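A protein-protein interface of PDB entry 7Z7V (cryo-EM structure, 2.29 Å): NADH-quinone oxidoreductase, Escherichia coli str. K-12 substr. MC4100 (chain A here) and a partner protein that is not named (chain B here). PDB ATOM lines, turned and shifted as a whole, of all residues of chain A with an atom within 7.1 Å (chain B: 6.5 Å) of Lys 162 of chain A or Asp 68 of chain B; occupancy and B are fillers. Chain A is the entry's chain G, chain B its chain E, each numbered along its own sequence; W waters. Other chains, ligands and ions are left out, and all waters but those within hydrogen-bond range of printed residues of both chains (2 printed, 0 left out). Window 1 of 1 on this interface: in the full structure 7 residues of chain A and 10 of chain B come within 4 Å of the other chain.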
ATOM      1  N   ARG A 156      35.141  21.360 -18.263  1.00  0.00           N
ATOM      2  CA  ARG A 156      35.178  20.929 -16.866  1.00  0.00           C
ATOM      3  C   ARG A 156      34.209  21.731 -16.009  1.00  0.00           C
ATOM      4  O   ARG A 156      33.556  21.174 -15.119  1.00  0.00           O
ATOM      5  CB  ARG A 156      36.588  21.070 -16.305  1.00  0.00           C
ATOM      6  CG  ARG A 156      37.406  19.808 -16.281  1.00  0.00           C
ATOM      7  CD  ARG A 156      38.795  20.122 -15.786  1.00  0.00           C
ATOM      8  NE  ARG A 156      39.533  18.937 -15.376  1.00  0.00           N
ATOM      9  CZ  ARG A 156      40.408  18.911 -14.383  1.00  0.00           C
ATOM     10  NH1 ARG A 156      40.670  19.989 -13.665  1.00  0.00           N
ATOM     11  NH2 ARG A 156      41.033  17.775 -14.100  1.00  0.00           N
ATOM     12  N   CYS A 157      34.112  23.038 -16.263  1.00  0.00           N
ATOM     13  CA  CYS A 157      33.294  23.917 -15.434  1.00  0.00           C
ATOM     14  C   CYS A 157      31.822  23.556 -15.523  1.00  0.00           C
ATOM     15  O   CYS A 157      31.142  23.452 -14.501  1.00  0.00           O
ATOM     16  CB  CYS A 157      33.486  25.373 -15.847  1.00  0.00           C
ATOM     17  SG  CYS A 157      33.191  25.691 -17.588  1.00  0.00           S
ATOM     18  N   VAL A 158      31.311  23.372 -16.741  1.00  0.00           N
ATOM     19  CA  VAL A 158      29.894  23.076 -16.898  1.00  0.00           C
ATOM     20  C   VAL A 158      29.583  21.680 -16.382  1.00  0.00           C
ATOM     21  O   VAL A 158      28.537  21.459 -15.768  1.00  0.00           O
ATOM     22  CB  VAL A 158      29.447  23.266 -18.359  1.00  0.00           C
ATOM     23  CG1 VAL A 158      29.307  24.741 -18.660  1.00  0.00           C
ATOM     24  CG2 VAL A 158      30.410  22.615 -19.328  1.00  0.00           C
ATOM     25  N   ARG A 159      30.499  20.731 -16.585  1.00  0.00           N
ATOM     26  CA  ARG A 159      30.282  19.375 -16.099  1.00  0.00           C
ATOM     27  C   ARG A 159      30.225  19.345 -14.578  1.00  0.00           C
ATOM     28  O   ARG A 159      29.281  18.797 -14.007  1.00  0.00           O
ATOM     29  CB  ARG A 159      31.362  18.443 -16.641  1.00  0.00           C
ATOM     30  CG  ARG A 159      31.166  18.146 -18.115  1.00  0.00           C
ATOM     31  CD  ARG A 159      31.769  16.842 -18.529  1.00  0.00           C
ATOM     32  NE  ARG A 159      33.152  16.682 -18.108  1.00  0.00           N
ATOM     33  CZ  ARG A 159      33.578  15.701 -17.327  1.00  0.00           C
ATOM     34  NH1 ARG A 159      32.746  14.800 -16.837  1.00  0.00           N
ATOM     35  NH2 ARG A 159      34.869  15.625 -17.026  1.00  0.00           N
ATOM     36  N   TYR A 160      31.161  20.031 -13.912  1.00  0.00           N
ATOM     37  CA  TYR A 160      31.106  20.127 -12.457  1.00  0.00           C
ATOM     38  C   TYR A 160      29.847  20.856 -11.995  1.00  0.00           C
ATOM     39  O   TYR A 160      29.049  20.304 -11.230  1.00  0.00           O
ATOM     40  CB  TYR A 160      32.351  20.835 -11.915  1.00  0.00           C
ATOM     41  CG  TYR A 160      32.129  21.384 -10.523  1.00  0.00           C
ATOM     42  CD1 TYR A 160      32.063  20.529  -9.431  1.00  0.00           C
ATOM     43  CD2 TYR A 160      31.946  22.745 -10.304  1.00  0.00           C
ATOM     44  CE1 TYR A 160      31.837  21.009  -8.171  1.00  0.00           C
ATOM     45  CE2 TYR A 160      31.713  23.230  -9.041  1.00  0.00           C
ATOM     46  CZ  TYR A 160      31.663  22.358  -7.979  1.00  0.00           C
ATOM     47  OH  TYR A 160      31.438  22.829  -6.717  1.00  0.00           O
ATOM     48  N   TYR A 161      29.621  22.063 -12.520  1.00  0.00           N
ATOM     49  CA  TYR A 161      28.579  22.951 -12.016  1.00  0.00           C
ATOM     50  C   TYR A 161      27.183  22.385 -12.237  1.00  0.00           C
ATOM     51  O   TYR A 161      26.334  22.467 -11.345  1.00  0.00           O
ATOM     52  CB  TYR A 161      28.715  24.317 -12.684  1.00  0.00           C
ATOM     53  CG  TYR A 161      28.064  25.464 -11.952  1.00  0.00           C
ATOM     54  CD1 TYR A 161      26.722  25.757 -12.140  1.00  0.00           C
ATOM     55  CD2 TYR A 161      28.793  26.261 -11.080  1.00  0.00           C
ATOM     56  CE1 TYR A 161      26.126  26.806 -11.488  1.00  0.00           C
ATOM     57  CE2 TYR A 161      28.200  27.314 -10.419  1.00  0.00           C
ATOM     58  CZ  TYR A 161      26.865  27.582 -10.629  1.00  0.00           C
ATOM     59  OH  TYR A 161      26.266  28.630  -9.977  1.00  0.00           O
ATOM     60  N   LYS A 162      26.925  21.796 -13.402  1.00  0.00           N
ATOM     61  CA  LYS A 162      25.607  21.255 -13.691  1.00  0.00           C
ATOM     62  C   LYS A 162      25.490  19.780 -13.329  1.00  0.00           C
ATOM     63  O   LYS A 162      24.568  19.395 -12.610  1.00  0.00           O
ATOM     64  CB  LYS A 162      25.272  21.454 -15.169  1.00  0.00           C
ATOM     65  CG  LYS A 162      25.305  22.888 -15.615  1.00  0.00           C
ATOM     66  CD  LYS A 162      25.367  22.968 -17.121  1.00  0.00           C
ATOM     67  CE  LYS A 162      23.980  22.878 -17.716  1.00  0.00           C
ATOM     68  NZ  LYS A 162      23.297  24.198 -17.741  1.00  0.00           N
ATOM     69  N   ASP A 163      26.380  18.931 -13.845  1.00  0.00           N
ATOM     70  CA  ASP A 163      26.216  17.507 -13.619  1.00  0.00           C
ATOM     71  C   ASP A 163      26.607  17.099 -12.205  1.00  0.00           C
ATOM     72  O   ASP A 163      26.006  16.172 -11.657  1.00  0.00           O
ATOM     73  CB  ASP A 163      27.028  16.727 -14.652  1.00  0.00           C
ATOM     74  CG  ASP A 163      26.760  17.193 -16.068  1.00  0.00           C
ATOM     75  OD1 ASP A 163      25.585  17.455 -16.394  1.00  0.00           O
ATOM     76  OD2 ASP A 163      27.719  17.302 -16.859  1.00  0.00           O
ATOM     77  N   TYR A 164      27.588  17.762 -11.590  1.00  0.00           N
ATOM     78  CA  TYR A 164      27.976  17.386 -10.235  1.00  0.00           C
ATOM     79  C   TYR A 164      27.231  18.205  -9.184  1.00  0.00           C
ATOM     80  O   TYR A 164      26.534  17.644  -8.335  1.00  0.00           O
ATOM     81  CB  TYR A 164      29.493  17.526 -10.057  1.00  0.00           C
ATOM     82  CG  TYR A 164      30.021  16.809  -8.837  1.00  0.00           C
ATOM     83  CD1 TYR A 164      30.046  17.433  -7.596  1.00  0.00           C
ATOM     84  CD2 TYR A 164      30.480  15.504  -8.920  1.00  0.00           C
ATOM     85  CE1 TYR A 164      30.511  16.781  -6.480  1.00  0.00           C
ATOM     86  CE2 TYR A 164      30.954  14.847  -7.808  1.00  0.00           C
ATOM     87  CZ  TYR A 164      30.969  15.490  -6.592  1.00  0.00           C
ATOM     88  OH  TYR A 164      31.435  14.838  -5.481  1.00  0.00           O
ATOM     89  N   ALA A 165      27.373  19.526  -9.225  1.00  0.00           N
ATOM     90  CA  ALA A 165      26.826  20.390  -8.187  1.00  0.00           C
ATOM     91  C   ALA A 165      25.364  20.752  -8.408  1.00  0.00           C
ATOM     92  O   ALA A 165      24.793  21.451  -7.564  1.00  0.00           O
ATOM     93  CB  ALA A 165      27.660  21.666  -8.075  1.00  0.00           C
ATOM     94  N   ASP A 166      24.765  20.312  -9.520  1.00  0.00           N
ATOM     95  CA  ASP A 166      23.358  20.557  -9.863  1.00  0.00           C
ATOM     96  C   ASP A 166      23.021  22.043  -9.946  1.00  0.00           C
ATOM     97  O   ASP A 166      21.881  22.442  -9.708  1.00  0.00           O
ATOM     98  CB  ASP A 166      22.405  19.848  -8.897  1.00  0.00           C
ATOM     99  CG  ASP A 166      22.492  18.340  -8.995  1.00  0.00           C
ATOM    100  OD1 ASP A 166      22.988  17.837 -10.022  1.00  0.00           O
ATOM    101  OD2 ASP A 166      22.064  17.653  -8.046  1.00  0.00           O
ATOM    102  N   GLY A 167      24.002  22.875 -10.283  1.00  0.00           N
ATOM    103  CA  GLY A 167      23.725  24.273 -10.516  1.00  0.00           C
ATOM    104  C   GLY A 167      23.023  24.491 -11.840  1.00  0.00           C
ATOM    105  O   GLY A 167      23.099  23.682 -12.762  1.00  0.00           O
ATOM    106  N   THR A 168      22.316  25.613 -11.936  1.00  0.00           N
ATOM    107  CA  THR A 168      21.498  25.887 -13.105  1.00  0.00           C
ATOM    108  C   THR A 168      21.917  27.109 -13.904  1.00  0.00           C
ATOM    109  O   THR A 168      21.500  27.230 -15.058  1.00  0.00           O
ATOM    110  CB  THR A 168      20.021  26.051 -12.705  1.00  0.00           C
ATOM    111  OG1 THR A 168      19.900  27.069 -11.707  1.00  0.00           O
ATOM    112  CG2 THR A 168      19.463  24.740 -12.159  1.00  0.00           C
ATOM    113  N   ASP A 169      22.728  28.004 -13.347  1.00  0.00           N
ATOM    114  CA  ASP A 169      22.980  29.296 -13.971  1.00  0.00           C
ATOM    115  C   ASP A 169      24.332  29.386 -14.668  1.00  0.00           C
ATOM    116  O   ASP A 169      24.760  30.489 -15.007  1.00  0.00           O
ATOM    117  CB  ASP A 169      22.853  30.415 -12.937  1.00  0.00           C
ATOM    118  CG  ASP A 169      23.770  30.223 -11.753  1.00  0.00           C
ATOM    119  OD1 ASP A 169      23.879  29.089 -11.255  1.00  0.00           O
ATOM    120  OD2 ASP A 169      24.377  31.214 -11.316  1.00  0.00           O
ATOM    121  N   LEU A 170      25.013  28.272 -14.888  1.00  0.00           N
ATOM    122  CA  LEU A 170      26.223  28.254 -15.696  1.00  0.00           C
ATOM    123  C   LEU A 170      26.027  27.290 -16.853  1.00  0.00           C
ATOM    124  O   LEU A 170      25.402  26.239 -16.697  1.00  0.00           O
ATOM    125  CB  LEU A 170      27.454  27.860 -14.874  1.00  0.00           C
ATOM    126  CG  LEU A 170      28.818  28.147 -15.505  1.00  0.00           C
ATOM    127  CD1 LEU A 170      29.353  29.493 -15.056  1.00  0.00           C
ATOM    128  CD2 LEU A 170      29.801  27.043 -15.180  1.00  0.00           C
ATOM    129  N   GLY A 171      26.546  27.660 -18.017  1.00  0.00           N
ATOM    130  CA  GLY A 171      26.349  26.866 -19.209  1.00  0.00           C
ATOM    131  C   GLY A 171      27.356  27.219 -20.280  1.00  0.00           C
ATOM    132  O   GLY A 171      28.219  28.085 -20.105  1.00  0.00           O
ATOM    133  N   VAL A 172      27.235  26.512 -21.400  1.00  0.00           N
ATOM    134  CA  VAL A 172      28.071  26.712 -22.573  1.00  0.00           C
ATOM    135  C   VAL A 172      27.185  27.211 -23.708  1.00  0.00           C
ATOM    136  O   VAL A 172      26.072  26.714 -23.911  1.00  0.00           O
ATOM    137  CB  VAL A 172      28.833  25.420 -22.952  1.00  0.00           C
ATOM    138  CG1 VAL A 172      27.899  24.223 -23.039  1.00  0.00           C
ATOM    139  CG2 VAL A 172      29.631  25.594 -24.237  1.00  0.00           C
ATOM    140  N   TYR A 173      27.664  28.227 -24.416  1.00  0.00           N
ATOM    141  CA  TYR A 173      26.920  28.914 -25.458  1.00  0.00           C
ATOM    142  C   TYR A 173      27.764  28.992 -26.720  1.00  0.00           C
ATOM    143  O   TYR A 173      28.978  28.791 -26.691  1.00  0.00           O
ATOM    144  CB  TYR A 173      26.500  30.312 -24.991  1.00  0.00           C
ATOM    145  CG  TYR A 173      26.055  30.310 -23.556  1.00  0.00           C
ATOM    146  CD1 TYR A 173      24.825  29.781 -23.200  1.00  0.00           C
ATOM    147  CD2 TYR A 173      26.880  30.787 -22.552  1.00  0.00           C
ATOM    148  CE1 TYR A 173      24.417  29.752 -21.891  1.00  0.00           C
ATOM    149  CE2 TYR A 173      26.481  30.762 -21.240  1.00  0.00           C
ATOM    150  CZ  TYR A 173      25.249  30.243 -20.915  1.00  0.00           C
ATOM    151  OH  TYR A 173      24.848  30.214 -19.609  1.00  0.00           O
ATOM    152  N   PRO A 184      24.004  32.990 -18.438  1.00  0.00           N
ATOM    153  CA  PRO A 184      23.256  33.608 -19.548  1.00  0.00           C
ATOM    154  C   PRO A 184      23.218  35.127 -19.492  1.00  0.00           C
ATOM    155  O   PRO A 184      22.972  35.758 -20.526  1.00  0.00           O
ATOM    156  CB  PRO A 184      21.852  33.000 -19.414  1.00  0.00           C
ATOM    157  CG  PRO A 184      21.769  32.512 -18.027  1.00  0.00           C
ATOM    158  CD  PRO A 184      23.145  32.104 -17.631  1.00  0.00           C
ATOM    159  N   LYS A 398      22.336  10.838  -7.458  1.00  0.00           N
ATOM    160  CA  LYS A 398      22.771  10.339  -8.774  1.00  0.00           C
ATOM    161  C   LYS A 398      23.168   8.858  -8.768  1.00  0.00           C
ATOM    162  O   LYS A 398      23.393   8.265  -9.847  1.00  0.00           O
ATOM    163  CB  LYS A 398      23.937  11.178  -9.291  1.00  0.00           C
ATOM    164  CG  LYS A 398      23.555  12.580  -9.703  1.00  0.00           C
ATOM    165  CD  LYS A 398      24.790  13.415  -9.971  1.00  0.00           C
ATOM    166  CE  LYS A 398      24.884  14.579  -9.018  1.00  0.00           C
ATOM    167  NZ  LYS A 398      24.284  15.793  -9.610  1.00  0.00           N
ATOM    168  N   ARG B  33      12.137  18.917 -22.227  1.00  0.00           N
ATOM    169  CA  ARG B  33      13.334  19.563 -22.761  1.00  0.00           C
ATOM    170  C   ARG B  33      13.434  19.402 -24.273  1.00  0.00           C
ATOM    171  O   ARG B  33      13.975  20.276 -24.958  1.00  0.00           O
ATOM    172  CB  ARG B  33      14.579  18.990 -22.080  1.00  0.00           C
ATOM    173  CG  ARG B  33      15.897  19.607 -22.514  1.00  0.00           C
ATOM    174  CD  ARG B  33      17.069  18.743 -22.111  1.00  0.00           C
ATOM    175  NE  ARG B  33      17.214  18.690 -20.663  1.00  0.00           N
ATOM    176  CZ  ARG B  33      17.824  19.614 -19.937  1.00  0.00           C
ATOM    177  NH1 ARG B  33      18.390  20.670 -20.496  1.00  0.00           N
ATOM    178  NH2 ARG B  33      17.863  19.480 -18.617  1.00  0.00           N
ATOM    179  N   SER B  36      12.545  22.298 -26.800  1.00  0.00           N
ATOM    180  CA  SER B  36      13.235  23.577 -26.648  1.00  0.00           C
ATOM    181  C   SER B  36      13.499  24.242 -27.992  1.00  0.00           C
ATOM    182  O   SER B  36      13.278  25.450 -28.150  1.00  0.00           O
ATOM    183  CB  SER B  36      14.541  23.380 -25.878  1.00  0.00           C
ATOM    184  OG  SER B  36      15.475  22.645 -26.643  1.00  0.00           O
ATOM    185  N   ILE B  55      14.093  33.714 -23.457  1.00  0.00           N
ATOM    186  CA  ILE B  55      14.891  32.610 -22.927  1.00  0.00           C
ATOM    187  C   ILE B  55      14.354  32.175 -21.570  1.00  0.00           C
ATOM    188  O   ILE B  55      14.084  30.990 -21.337  1.00  0.00           O
ATOM    189  CB  ILE B  55      16.372  33.020 -22.839  1.00  0.00           C
ATOM    190  CG1 ILE B  55      16.904  33.399 -24.223  1.00  0.00           C
ATOM    191  CG2 ILE B  55      17.202  31.913 -22.207  1.00  0.00           C
ATOM    192  CD1 ILE B  55      16.910  32.259 -25.210  1.00  0.00           C
ATOM    193  N   ILE B  64      13.178  23.720 -17.579  1.00  0.00           N
ATOM    194  CA  ILE B  64      14.620  23.520 -17.712  1.00  0.00           C
ATOM    195  C   ILE B  64      15.291  24.847 -17.389  1.00  0.00           C
ATOM    196  O   ILE B  64      14.634  25.900 -17.402  1.00  0.00           O
ATOM    197  CB  ILE B  64      14.998  22.987 -19.115  1.00  0.00           C
ATOM    198  CG1 ILE B  64      14.548  23.949 -20.213  1.00  0.00           C
ATOM    199  CG2 ILE B  64      14.421  21.599 -19.330  1.00  0.00           C
ATOM    200  CD1 ILE B  64      14.964  23.507 -21.592  1.00  0.00           C
ATOM    201  N   PRO B  65      16.581  24.834 -17.034  1.00  0.00           N
ATOM    202  CA  PRO B  65      17.270  26.098 -16.739  1.00  0.00           C
ATOM    203  C   PRO B  65      17.380  27.009 -17.954  1.00  0.00           C
ATOM    204  O   PRO B  65      17.394  26.561 -19.101  1.00  0.00           O
ATOM    205  CB  PRO B  65      18.656  25.642 -16.270  1.00  0.00           C
ATOM    206  CG  PRO B  65      18.446  24.295 -15.751  1.00  0.00           C
ATOM    207  CD  PRO B  65      17.383  23.677 -16.596  1.00  0.00           C
ATOM    208  N   ALA B  66      17.455  28.314 -17.678  1.00  0.00           N
ATOM    209  CA  ALA B  66      17.614  29.297 -18.743  1.00  0.00           C
ATOM    210  C   ALA B  66      18.975  29.190 -19.415  1.00  0.00           C
ATOM    211  O   ALA B  66      19.110  29.553 -20.587  1.00  0.00           O
ATOM    212  CB  ALA B  66      17.404  30.705 -18.195  1.00  0.00           C
ATOM    213  N   SER B  67      19.986  28.700 -18.694  1.00  0.00           N
ATOM    214  CA  SER B  67      21.295  28.490 -19.302  1.00  0.00           C
ATOM    215  C   SER B  67      21.231  27.425 -20.392  1.00  0.00           C
ATOM    216  O   SER B  67      21.887  27.555 -21.428  1.00  0.00           O
ATOM    217  CB  SER B  67      22.324  28.116 -18.234  1.00  0.00           C
ATOM    218  OG  SER B  67      21.923  26.973 -17.503  1.00  0.00           O
ATOM    219  N   ASP B  68      20.423  26.381 -20.191  1.00  0.00           N
ATOM    220  CA  ASP B  68      20.244  25.364 -21.226  1.00  0.00           C
ATOM    221  C   ASP B  68      19.518  25.915 -22.449  1.00  0.00           C
ATOM    222  O   ASP B  68      19.890  25.602 -23.588  1.00  0.00           O
ATOM    223  CB  ASP B  68      19.497  24.160 -20.659  1.00  0.00           C
ATOM    224  CG  ASP B  68      20.311  23.406 -19.631  1.00  0.00           C
ATOM    225  OD1 ASP B  68      21.549  23.381 -19.771  1.00  0.00           O
ATOM    226  OD2 ASP B  68      19.724  22.822 -18.700  1.00  0.00           O
ATOM    227  N   VAL B  69      18.485  26.733 -22.235  1.00  0.00           N
ATOM    228  CA  VAL B  69      17.760  27.334 -23.353  1.00  0.00           C
ATOM    229  C   VAL B  69      18.668  28.272 -24.135  1.00  0.00           C
ATOM    230  O   VAL B  69      18.658  28.278 -25.369  1.00  0.00           O
ATOM    231  CB  VAL B  69      16.495  28.055 -22.854  1.00  0.00           C
ATOM    232  CG1 VAL B  69      15.721  28.646 -24.022  1.00  0.00           C
ATOM    233  CG2 VAL B  69      15.617  27.105 -22.080  1.00  0.00           C
ATOM    234  N   GLU B  70      19.478  29.068 -23.432  1.00  0.00           N
ATOM    235  CA  GLU B  70      20.403  29.958 -24.123  1.00  0.00           C
ATOM    236  C   GLU B  70      21.512  29.189 -24.832  1.00  0.00           C
ATOM    237  O   GLU B  70      21.935  29.590 -25.922  1.00  0.00           O
ATOM    238  CB  GLU B  70      20.980  30.984 -23.144  1.00  0.00           C
ATOM    239  CG  GLU B  70      22.027  31.925 -23.733  1.00  0.00           C
ATOM    240  CD  GLU B  70      21.440  33.128 -24.457  1.00  0.00           C
ATOM    241  OE1 GLU B  70      20.507  32.962 -25.268  1.00  0.00           O
ATOM    242  OE2 GLU B  70      21.924  34.254 -24.222  1.00  0.00           O
ATOM    243  N   GLY B  71      21.974  28.076 -24.254  1.00  0.00           N
ATOM    244  CA  GLY B  71      22.942  27.241 -24.945  1.00  0.00           C
ATOM    245  C   GLY B  71      22.392  26.654 -26.231  1.00  0.00           C
ATOM    246  O   GLY B  71      23.082  26.620 -27.253  1.00  0.00           O
ATOM    247  N   VAL B  72      21.132  26.218 -26.201  1.00  0.00           N
ATOM    248  CA  VAL B  72      20.480  25.730 -27.414  1.00  0.00           C
ATOM    249  C   VAL B  72      20.319  26.859 -28.429  1.00  0.00           C
ATOM    250  O   VAL B  72      20.659  26.704 -29.604  1.00  0.00           O
ATOM    251  CB  VAL B  72      19.129  25.077 -27.069  1.00  0.00           C
ATOM    252  CG1 VAL B  72      18.316  24.842 -28.320  1.00  0.00           C
ATOM    253  CG2 VAL B  72      19.350  23.774 -26.336  1.00  0.00           C
ATOM    254  N   ALA B  73      19.838  28.022 -27.980  1.00  0.00           N
ATOM    255  CA  ALA B  73      19.551  29.125 -28.896  1.00  0.00           C
ATOM    256  C   ALA B  73      20.816  29.655 -29.559  1.00  0.00           C
ATOM    257  O   ALA B  73      20.804  29.995 -30.747  1.00  0.00           O
ATOM    258  CB  ALA B  73      18.828  30.247 -28.154  1.00  0.00           C
HETATM  259  O   HOH W   1      20.097  29.700 -15.661  1.00  0.00           O
HETATM  260  O   HOH W   2      24.390  25.545 -22.098  1.00  0.00           O
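Water W2 lies within hydrogen-bond range of O of Val 172 of chain A and O of Ser 67 of chain B. Water W1 bridges the backbone carbonyl oxygen (O) of Thr 168 of chain A (2.9 Å) and the backbone NH (N) of Ser 67 of chain B (3.2 Å).
O of Thr 168 of chain A touches CB of Pro 65 of chain B, at 3.5 Å. Leu 170 of chain A touches Ser 67 of chain B. Val 172 of chain A touches Gly 71 of chain B (O to CA, 3.3 Å). Tyr 173 of chain A touches Ser 67 of chain B (CE1 to O, 3.4 Å). CD1 of Tyr 173 of chain A touches CG of Glu 70 of chain B, 3.6 Å away. N of Gly 71 of chain B touches CD1 of Tyr 173 of chain A (3.5 Å).
Printed residues of chain A that touch a printed residue of chain B: Lys 162, Thr 168, Leu 170, Val 172 and Tyr 173. Of the 13 printed residues of chain B, 5 touch a printed residue of chain A. Printed residues of chain B that touch a printed residue of chain A: Pro 65, Ser 67, Asp 68, Glu 70 and Gly 71. Hydrophobic or aromatic side chains of chain B within 4 Å of the printed part of chain A: Pro 65. Among the printed residues, 9 pairs touch across the chains. Among the printed residues, Asp or Glu carboxylates within 4 Å of a Lys or Arg side-chain nitrogen of the other chain: Lys 162 of chain A with Asp 68 of chain B.
NH1 of Arg 33 of chain B lies within salt-bridge range of OD2 of Asp 68 of chain B (3.1 Å). The side-chain hydroxyl of Tyr 173 of chain A sits at hydrogen-bond distance from the backbone NH of Gly 171 of chain A, at 3.5 Å. O of Leu 170 of chain A sits at hydrogen-bond distance from NZ of Lys 162 of chain A (3.1 Å).
Lys 162 of chain A touches two residues of chain B. Of the printed residues of chain B, Tyr 173 of chain A touches Ser 67 (3.4 Å), Glu 70 (3.6 Å) and Gly 71 (3.5 Å). Printed residues of chain A within 4 Å of Ser 67 of chain B: Lys 162 (3.1 Å), Thr 168 (2.5 Å), Leu 170 (3.6 Å) and Tyr 173 (3.4 Å). Printed residues of chain A within 4 Å of Glu 70 of chain B: Tyr 173 (3.6 Å). Asp 163 of chain A touches none of the printed residues of chain B. Pro 184 of chain A touches none of the printed residues of chain B. The nearest residue of chain B that does not touch Lys 162 of chain A is Pro 65 of chain B (5.1 Å). The nearest residue of chain A that does not touch Asp 68 of chain B is Thr 168 of chain A (5.3 Å). The nearest printed residue of chain A that does not touch Glu 70 of chain B is Pro 184 of chain A (4.1 Å).
OG of Ser 67 of chain B sits at hydrogen-bond distance from O of Thr 168 of chain A. NZ of Lys 162 of chain A is in salt-bridge range of OD1 of Asp 68 of chain B (2.8 Å). The side-chain amino group (NZ) of Lys 162 of chain A lies within hydrogen-bond range of the side-chain hydroxyl (OG) of Ser 67 of chain B, 3.1 Å away.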
